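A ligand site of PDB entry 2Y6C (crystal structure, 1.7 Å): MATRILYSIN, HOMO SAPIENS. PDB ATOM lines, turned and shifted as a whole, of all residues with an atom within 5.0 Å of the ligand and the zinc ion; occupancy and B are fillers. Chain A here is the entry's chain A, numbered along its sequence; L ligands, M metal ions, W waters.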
ATOM      1  N   PHE A   5       7.445  -0.145  13.723  1.00  0.00           N
ATOM      2  CA  PHE A   5       6.246  -0.979  13.623  1.00  0.00           C
ATOM      3  C   PHE A   5       5.750  -1.015  12.184  1.00  0.00           C
ATOM      4  O   PHE A   5       5.967  -0.071  11.413  1.00  0.00           O
ATOM      5  CB  PHE A   5       5.139  -0.481  14.551  1.00  0.00           C
ATOM      6  CG  PHE A   5       5.296  -0.915  15.982  1.00  0.00           C
ATOM      7  CD1 PHE A   5       4.750  -2.112  16.432  1.00  0.00           C
ATOM      8  CD2 PHE A   5       5.982  -0.128  16.898  1.00  0.00           C
ATOM      9  CE1 PHE A   5       4.894  -2.518  17.742  1.00  0.00           C
ATOM     10  CE2 PHE A   5       6.135  -0.527  18.217  1.00  0.00           C
ATOM     11  CZ  PHE A   5       5.591  -1.722  18.639  1.00  0.00           C
ATOM     12  N   ASN A  81       6.908 -16.275  32.392  1.00  0.00           N
ATOM     13  CA  ASN A  81       6.416 -16.082  31.032  1.00  0.00           C
ATOM     14  C   ASN A  81       6.414 -14.604  30.637  1.00  0.00           C
ATOM     15  O   ASN A  81       7.441 -13.956  30.735  1.00  0.00           O
ATOM     16  CB  ASN A  81       5.090 -16.809  30.810  1.00  0.00           C
ATOM     17  CG  ASN A  81       5.264 -18.329  30.752  1.00  0.00           C
ATOM     18  OD1 ASN A  81       4.471 -19.090  31.300  1.00  0.00           O
ATOM     19  ND2 ASN A  81       6.331 -18.774  30.095  1.00  0.00           N
ATOM     20  N   THR A  82       5.273 -14.053  30.203  1.00  0.00           N
ATOM     21  CA  THR A  82       5.255 -12.639  29.796  1.00  0.00           C
ATOM     22  C   THR A  82       5.424 -11.696  30.988  1.00  0.00           C
ATOM     23  O   THR A  82       4.804 -11.904  32.030  1.00  0.00           O
ATOM     24  CB  THR A  82       3.985 -12.279  29.008  1.00  0.00           C
ATOM     25  OG1 THR A  82       3.939 -13.074  27.819  1.00  0.00           O
ATOM     26  CG2 THR A  82       4.015 -10.820  28.607  1.00  0.00           C
ATOM     27  N   LEU A  83       6.260 -10.665  30.823  1.00  0.00           N
ATOM     28  CA  LEU A  83       6.567  -9.731  31.917  1.00  0.00           C
ATOM     29  C   LEU A  83       5.894  -8.385  31.741  1.00  0.00           C
ATOM     30  O   LEU A  83       5.598  -7.693  32.718  1.00  0.00           O
ATOM     31  CB  LEU A  83       8.077  -9.473  31.957  1.00  0.00           C
ATOM     32  CG  LEU A  83       8.992 -10.692  31.872  1.00  0.00           C
ATOM     33  CD1 LEU A  83      10.450 -10.232  31.808  1.00  0.00           C
ATOM     34  CD2 LEU A  83       8.749 -11.625  33.018  1.00  0.00           C
ATOM     35  N   ALA A  84       5.707  -7.984  30.484  1.00  0.00           N
ATOM     36  CA  ALA A  84       5.138  -6.695  30.155  1.00  0.00           C
ATOM     37  C   ALA A  84       4.910  -6.594  28.664  1.00  0.00           C
ATOM     38  O   ALA A  84       5.409  -7.408  27.883  1.00  0.00           O
ATOM     39  CB  ALA A  84       6.101  -5.574  30.592  1.00  0.00           C
ATOM     40  N   HIS A  85       4.146  -5.580  28.276  1.00  0.00           N
ATOM     41  CA  HIS A  85       3.892  -5.295  26.887  1.00  0.00           C
ATOM     42  C   HIS A  85       3.466  -3.837  26.705  1.00  0.00           C
ATOM     43  O   HIS A  85       3.081  -3.149  27.663  1.00  0.00           O
ATOM     44  CB  HIS A  85       2.897  -6.284  26.236  1.00  0.00           C
ATOM     45  CG  HIS A  85       1.533  -6.321  26.873  1.00  0.00           C
ATOM     46  ND1 HIS A  85       0.940  -7.502  27.264  1.00  0.00           N
ATOM     47  CD2 HIS A  85       0.656  -5.333  27.165  1.00  0.00           C
ATOM     48  CE1 HIS A  85      -0.259  -7.245  27.767  1.00  0.00           C
ATOM     49  NE2 HIS A  85      -0.456  -5.940  27.717  1.00  0.00           N
ATOM     50  N   ALA A  86       3.605  -3.358  25.467  1.00  0.00           N
ATOM     51  CA  ALA A  86       3.271  -1.972  25.144  1.00  0.00           C
ATOM     52  C   ALA A  86       2.801  -1.915  23.706  1.00  0.00           C
ATOM     53  O   ALA A  86       3.134  -2.785  22.904  1.00  0.00           O
ATOM     54  CB  ALA A  86       4.468  -1.046  25.364  1.00  0.00           C
ATOM     55  N   TRP A 105       9.697  -6.512  40.689  1.00  0.00           N
ATOM     56  CA  TRP A 105      10.306  -5.330  40.057  1.00  0.00           C
ATOM     57  C   TRP A 105      11.201  -4.608  41.053  1.00  0.00           C
ATOM     58  O   TRP A 105      10.870  -4.540  42.230  1.00  0.00           O
ATOM     59  CB  TRP A 105       9.212  -4.381  39.545  1.00  0.00           C
ATOM     60  CG  TRP A 105       8.264  -5.088  38.596  1.00  0.00           C
ATOM     61  CD1 TRP A 105       7.109  -5.725  38.916  1.00  0.00           C
ATOM     62  CD2 TRP A 105       8.465  -5.290  37.190  1.00  0.00           C
ATOM     63  NE1 TRP A 105       6.546  -6.288  37.787  1.00  0.00           N
ATOM     64  CE2 TRP A 105       7.357  -6.032  36.711  1.00  0.00           C
ATOM     65  CE3 TRP A 105       9.439  -4.880  36.276  1.00  0.00           C
ATOM     66  CZ2 TRP A 105       7.221  -6.397  35.373  1.00  0.00           C
ATOM     67  CZ3 TRP A 105       9.301  -5.232  34.953  1.00  0.00           C
ATOM     68  CH2 TRP A 105       8.201  -5.976  34.503  1.00  0.00           C
ATOM     69  N   ILE A 113      13.366  -7.617  38.440  1.00  0.00           N
ATOM     70  CA  ILE A 113      13.581  -7.114  37.108  1.00  0.00           C
ATOM     71  C   ILE A 113      13.842  -5.629  37.284  1.00  0.00           C
ATOM     72  O   ILE A 113      13.102  -4.951  37.998  1.00  0.00           O
ATOM     73  CB  ILE A 113      12.318  -7.231  36.248  1.00  0.00           C
ATOM     74  CG1 ILE A 113      11.806  -8.665  36.188  1.00  0.00           C
ATOM     75  CG2 ILE A 113      12.575  -6.672  34.845  1.00  0.00           C
ATOM     76  CD1 ILE A 113      10.360  -8.762  35.666  1.00  0.00           C
ATOM     77  N   TYR A 117      15.155  -0.235  33.182  1.00  0.00           N
ATOM     78  CA  TYR A 117      15.458  -0.851  31.898  1.00  0.00           C
ATOM     79  C   TYR A 117      14.168  -1.330  31.261  1.00  0.00           C
ATOM     80  O   TYR A 117      13.912  -1.073  30.083  1.00  0.00           O
ATOM     81  CB  TYR A 117      16.445  -2.001  32.042  1.00  0.00           C
ATOM     82  CG  TYR A 117      16.909  -2.572  30.721  1.00  0.00           C
ATOM     83  CD1 TYR A 117      16.174  -3.547  30.059  1.00  0.00           C
ATOM     84  CD2 TYR A 117      18.101  -2.135  30.127  1.00  0.00           C
ATOM     85  CE1 TYR A 117      16.599  -4.061  28.831  1.00  0.00           C
ATOM     86  CE2 TYR A 117      18.526  -2.657  28.907  1.00  0.00           C
ATOM     87  CZ  TYR A 117      17.769  -3.621  28.272  1.00  0.00           C
ATOM     88  OH  TYR A 117      18.185  -4.157  27.050  1.00  0.00           O
ATOM     89  N   ALA A 118      13.347  -2.036  32.038  1.00  0.00           N
ATOM     90  CA  ALA A 118      12.092  -2.541  31.494  1.00  0.00           C
ATOM     91  C   ALA A 118      11.221  -1.396  30.966  1.00  0.00           C
ATOM     92  O   ALA A 118      10.673  -1.478  29.883  1.00  0.00           O
ATOM     93  CB  ALA A 118      11.330  -3.380  32.529  1.00  0.00           C
ATOM     94  N   ALA A 119      11.090  -0.322  31.744  1.00  0.00           N
ATOM     95  CA  ALA A 119      10.294   0.821  31.306  1.00  0.00           C
ATOM     96  C   ALA A 119      10.849   1.465  30.033  1.00  0.00           C
ATOM     97  O   ALA A 119      10.093   1.898  29.169  1.00  0.00           O
ATOM     98  CB  ALA A 119      10.193   1.854  32.431  1.00  0.00           C
ATOM     99  N   HIS A 121      12.558  -0.035  27.658  1.00  0.00           N
ATOM    100  CA  HIS A 121      12.231  -0.963  26.556  1.00  0.00           C
ATOM    101  C   HIS A 121      10.767  -0.827  26.147  1.00  0.00           C
ATOM    102  O   HIS A 121      10.453  -0.616  24.977  1.00  0.00           O
ATOM    103  CB  HIS A 121      12.554  -2.410  26.931  1.00  0.00           C
ATOM    104  CG  HIS A 121      12.239  -3.396  25.854  1.00  0.00           C
ATOM    105  ND1 HIS A 121      13.200  -3.906  25.015  1.00  0.00           N
ATOM    106  CD2 HIS A 121      11.066  -3.963  25.468  1.00  0.00           C
ATOM    107  CE1 HIS A 121      12.643  -4.748  24.160  1.00  0.00           C
ATOM    108  NE2 HIS A 121      11.344  -4.800  24.416  1.00  0.00           N
ATOM    109  N   GLU A 122       9.856  -0.946  27.119  1.00  0.00           N
ATOM    110  CA  GLU A 122       8.415  -0.831  26.838  1.00  0.00           C
ATOM    111  C   GLU A 122       8.018   0.531  26.275  1.00  0.00           C
ATOM    112  O   GLU A 122       7.222   0.612  25.343  1.00  0.00           O
ATOM    113  CB  GLU A 122       7.584  -1.119  28.088  1.00  0.00           C
ATOM    114  CG  GLU A 122       7.752  -2.521  28.648  1.00  0.00           C
ATOM    115  CD  GLU A 122       7.488  -3.592  27.611  1.00  0.00           C
ATOM    116  OE1 GLU A 122       6.519  -3.436  26.822  1.00  0.00           O
ATOM    117  OE2 GLU A 122       8.220  -4.617  27.577  1.00  0.00           O
ATOM    118  N   HIS A 125       8.665   0.901  22.712  1.00  0.00           N
ATOM    119  CA  HIS A 125       7.536   0.441  21.888  1.00  0.00           C
ATOM    120  C   HIS A 125       6.418   1.487  21.835  1.00  0.00           C
ATOM    121  O   HIS A 125       5.824   1.721  20.777  1.00  0.00           O
ATOM    122  CB  HIS A 125       6.931  -0.891  22.411  1.00  0.00           C
ATOM    123  CG  HIS A 125       7.845  -2.066  22.300  1.00  0.00           C
ATOM    124  ND1 HIS A 125       8.480  -2.416  21.125  1.00  0.00           N
ATOM    125  CD2 HIS A 125       8.162  -3.034  23.202  1.00  0.00           C
ATOM    126  CE1 HIS A 125       9.180  -3.521  21.318  1.00  0.00           C
ATOM    127  NE2 HIS A 125       8.996  -3.919  22.573  1.00  0.00           N
ATOM    128  N   HIS A 131      11.781  -4.297  17.689  1.00  0.00           N
ATOM    129  CA  HIS A 131      12.976  -4.917  18.256  1.00  0.00           C
ATOM    130  C   HIS A 131      14.212  -4.780  17.370  1.00  0.00           C
ATOM    131  O   HIS A 131      14.120  -4.738  16.131  1.00  0.00           O
ATOM    132  CB  HIS A 131      12.742  -6.404  18.594  1.00  0.00           C
ATOM    133  CG  HIS A 131      11.785  -6.613  19.720  1.00  0.00           C
ATOM    134  ND1 HIS A 131      10.716  -7.477  19.648  1.00  0.00           N
ATOM    135  CD2 HIS A 131      11.709  -6.038  20.945  1.00  0.00           C
ATOM    136  CE1 HIS A 131      10.039  -7.445  20.779  1.00  0.00           C
ATOM    137  NE2 HIS A 131      10.628  -6.571  21.582  1.00  0.00           N
ATOM    138  N   MET A 139      16.407  -2.075  22.855  1.00  0.00           N
ATOM    139  CA  MET A 139      15.289  -2.682  22.122  1.00  0.00           C
ATOM    140  C   MET A 139      15.538  -4.114  21.620  1.00  0.00           C
ATOM    141  O   MET A 139      14.740  -4.662  20.867  1.00  0.00           O
ATOM    142  CB  MET A 139      14.800  -1.779  20.978  1.00  0.00           C
ATOM    143  CG  MET A 139      14.306  -0.406  21.440  1.00  0.00           C
ATOM    144  SD  MET A 139      13.003  -0.506  22.715  1.00  0.00           S
ATOM    145  CE  MET A 139      11.821  -1.595  21.918  1.00  0.00           C
ATOM    146  N   TYR A 140      16.652  -4.716  22.041  1.00  0.00           N
ATOM    147  CA  TYR A 140      16.919  -6.115  21.713  1.00  0.00           C
ATOM    148  C   TYR A 140      15.751  -6.884  22.322  1.00  0.00           C
ATOM    149  O   TYR A 140      15.233  -6.499  23.372  1.00  0.00           O
ATOM    150  CB  TYR A 140      18.254  -6.552  22.307  1.00  0.00           C
ATOM    151  CG  TYR A 140      18.809  -7.863  21.811  1.00  0.00           C
ATOM    152  CD1 TYR A 140      19.204  -8.025  20.483  1.00  0.00           C
ATOM    153  CD2 TYR A 140      19.021  -8.920  22.686  1.00  0.00           C
ATOM    154  CE1 TYR A 140      19.750  -9.218  20.029  1.00  0.00           C
ATOM    155  CE2 TYR A 140      19.567 -10.121  22.239  1.00  0.00           C
ATOM    156  CZ  TYR A 140      19.931 -10.264  20.918  1.00  0.00           C
ATOM    157  OH  TYR A 140      20.475 -11.451  20.485  1.00  0.00           O
ATOM    158  N   PRO A 141      15.312  -7.981  21.677  1.00  0.00           N
ATOM    159  CA  PRO A 141      14.099  -8.658  22.133  1.00  0.00           C
ATOM    160  C   PRO A 141      14.139  -9.315  23.521  1.00  0.00           C
ATOM    161  O   PRO A 141      13.081  -9.580  24.084  1.00  0.00           O
ATOM    162  CB  PRO A 141      13.827  -9.697  21.042  1.00  0.00           C
ATOM    163  CG  PRO A 141      15.136  -9.880  20.338  1.00  0.00           C
ATOM    164  CD  PRO A 141      15.861  -8.573  20.438  1.00  0.00           C
ATOM    165  N   THR A 142      15.319  -9.573  24.061  1.00  0.00           N
ATOM    166  CA  THR A 142      15.386 -10.244  25.356  1.00  0.00           C
ATOM    167  C   THR A 142      16.017  -9.386  26.459  1.00  0.00           C
ATOM    168  O   THR A 142      16.816  -8.484  26.176  1.00  0.00           O
ATOM    169  CB  THR A 142      16.120 -11.603  25.216  1.00  0.00           C
ATOM    170  OG1 THR A 142      17.413 -11.397  24.635  1.00  0.00           O
ATOM    171  CG2 THR A 142      15.320 -12.523  24.298  1.00  0.00           C
ATOM    172  N   TYR A 143      15.637  -9.658  27.703  1.00  0.00           N
ATOM    173  CA  TYR A 143      16.170  -8.936  28.861  1.00  0.00           C
ATOM    174  C   TYR A 143      17.474  -9.586  29.320  1.00  0.00           C
ATOM    175  O   TYR A 143      18.486  -8.915  29.490  1.00  0.00           O
ATOM    176  CB  TYR A 143      15.152  -8.936  30.012  1.00  0.00           C
ATOM    177  CG  TYR A 143      15.599  -8.306  31.322  1.00  0.00           C
ATOM    178  CD1 TYR A 143      16.333  -9.029  32.266  1.00  0.00           C
ATOM    179  CD2 TYR A 143      15.257  -6.995  31.641  1.00  0.00           C
ATOM    180  CE1 TYR A 143      16.729  -8.451  33.471  1.00  0.00           C
ATOM    181  CE2 TYR A 143      15.644  -6.416  32.831  1.00  0.00           C
ATOM    182  CZ  TYR A 143      16.380  -7.145  33.753  1.00  0.00           C
ATOM    183  OH  TYR A 143      16.756  -6.561  34.950  1.00  0.00           O
HETATM  184  N1  LIG L   1       7.116  -8.658  26.291  1.00  0.00           N
HETATM  185  C1  LIG L   1       7.417  -8.577  24.859  1.00  0.00           C
HETATM  186  C2  LIG L   1       8.117  -7.250  24.725  1.00  0.00           C
HETATM  187  O1  LIG L   1       7.946  -6.265  25.417  1.00  0.00           O
HETATM  188  C3  LIG L   1       6.085  -8.502  24.156  1.00  0.00           C
HETATM  189  C4  LIG L   1       5.916  -7.201  23.512  1.00  0.00           C
HETATM  190  C5  LIG L   1       5.581  -6.014  24.114  1.00  0.00           C
HETATM  191  C6  LIG L   1       6.106  -6.951  22.120  1.00  0.00           C
HETATM  192  N2  LIG L   1       5.551  -5.062  23.136  1.00  0.00           N
HETATM  193  C7  LIG L   1       5.866  -5.603  21.922  1.00  0.00           C
HETATM  194  C8  LIG L   1       6.443  -7.764  21.067  1.00  0.00           C
HETATM  195  C9  LIG L   1       5.939  -4.985  20.688  1.00  0.00           C
HETATM  196  C10 LIG L   1       6.526  -7.159  19.833  1.00  0.00           C
HETATM  197  C11 LIG L   1       6.285  -5.820  19.655  1.00  0.00           C
HETATM  198  O2  LIG L   1       9.007  -7.293  23.720  1.00  0.00           O
HETATM  199  S1  LIG L   1       8.193  -9.604  27.213  1.00  0.00           S
HETATM  200  C12 LIG L   1      10.826  -6.941  28.634  1.00  0.00           C
HETATM  201  C13 LIG L   1      10.848  -6.011  29.796  1.00  0.00           C
HETATM  202  C14 LIG L   1       9.637  -8.594  27.425  1.00  0.00           C
HETATM  203  C15 LIG L   1       9.708  -7.718  28.479  1.00  0.00           C
HETATM  204  O3  LIG L   1       8.636 -10.756  26.457  1.00  0.00           O
HETATM  205  O4  LIG L   1       7.605  -9.813  28.526  1.00  0.00           O
HETATM  206  C16 LIG L   1      11.882  -7.054  27.749  1.00  0.00           C
HETATM  207  C17 LIG L   1      10.674  -8.714  26.531  1.00  0.00           C
HETATM  208  F1  LIG L   1       9.760  -6.163  30.591  1.00  0.00           F
HETATM  209  F2  LIG L   1      10.803  -4.706  29.415  1.00  0.00           F
HETATM  210  F3  LIG L   1      11.927  -6.183  30.597  1.00  0.00           F
HETATM  211  C18 LIG L   1      11.802  -7.944  26.693  1.00  0.00           C
HETATM  212 CL1  LIG L   1      13.323  -6.105  27.907  1.00  0.00          CL
HETATM  213 ZN    ZN M   1       9.951  -5.646  23.303  1.00  0.00          ZN
HETATM  214  O   HOH W   1      10.395  -9.783  23.122  1.00  0.00           O
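The zinc ion is bound by an oxygen (O2) of the ligand (1.9 Å), a ring nitrogen (NE2) of His 121 (2.0 Å), a ring nitrogen (NE2) of His 131 (2.1 Å) and a ring nitrogen (NE2) of His 125 (2.1 Å).
The zinc ion has four donor atoms within binding distance.
An oxygen (O1) of the ligand sits close to the side-chain carboxylate (OE2) of Glu 122, at 2.7 Å.
A nitrogen (N2) of the ligand lies within hydrogen-bond range of the backbone carbonyl oxygen (O) of Ala 86, at 3.3 Å.
The backbone NH (N) of Ala 84 is in hydrogen-bond range of an oxygen (O4) of the ligand (3.3 Å).
N of Leu 83 sits at hydrogen-bond distance from O4 of the ligand, at 2.8 Å.
O of Ala 84 sits at hydrogen-bond distance from N1 of the ligand, at 2.6 Å.
A fluorine (F2) of the ligand sits close to the backbone carbonyl oxygen of Ala 118 (3.3 Å).
Phe 5 touches the ligand.
CG2 of Thr 82 touches O4 of the ligand, at 3.7 Å.
His 85 touches the ligand.
CE1 of Tyr 117 touches CL1 of the ligand, 3.97 Å away.
Pro 141 touches the ligand.
Tyr 143 touches the ligand (CD2 to F3, 3.6 Å).
Hydrophobic or aromatic side chains within 4 Å of the ligand: Phe 5, Leu 83, Ala 84, His 85, Tyr 117, Ala 118, His 121, His 125, His 131 and Tyr 143.
14 residues have an atom within 4 Å of the ligand: Phe 5, Thr 82, Leu 83, Ala 84, His 85, Ala 86, Tyr 117, Ala 118, His 121, Glu 122, His 125, His 131, Pro 141 and Tyr 143.
The nearest printed residue that does not touch the ligand is Trp 105 (4.2 Å).
N of Ala 86 lies within hydrogen-bond range of OE1 of Glu 122.
Three residues have an atom within 4 Å of the zinc ion: His 121, His 125 and His 131.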
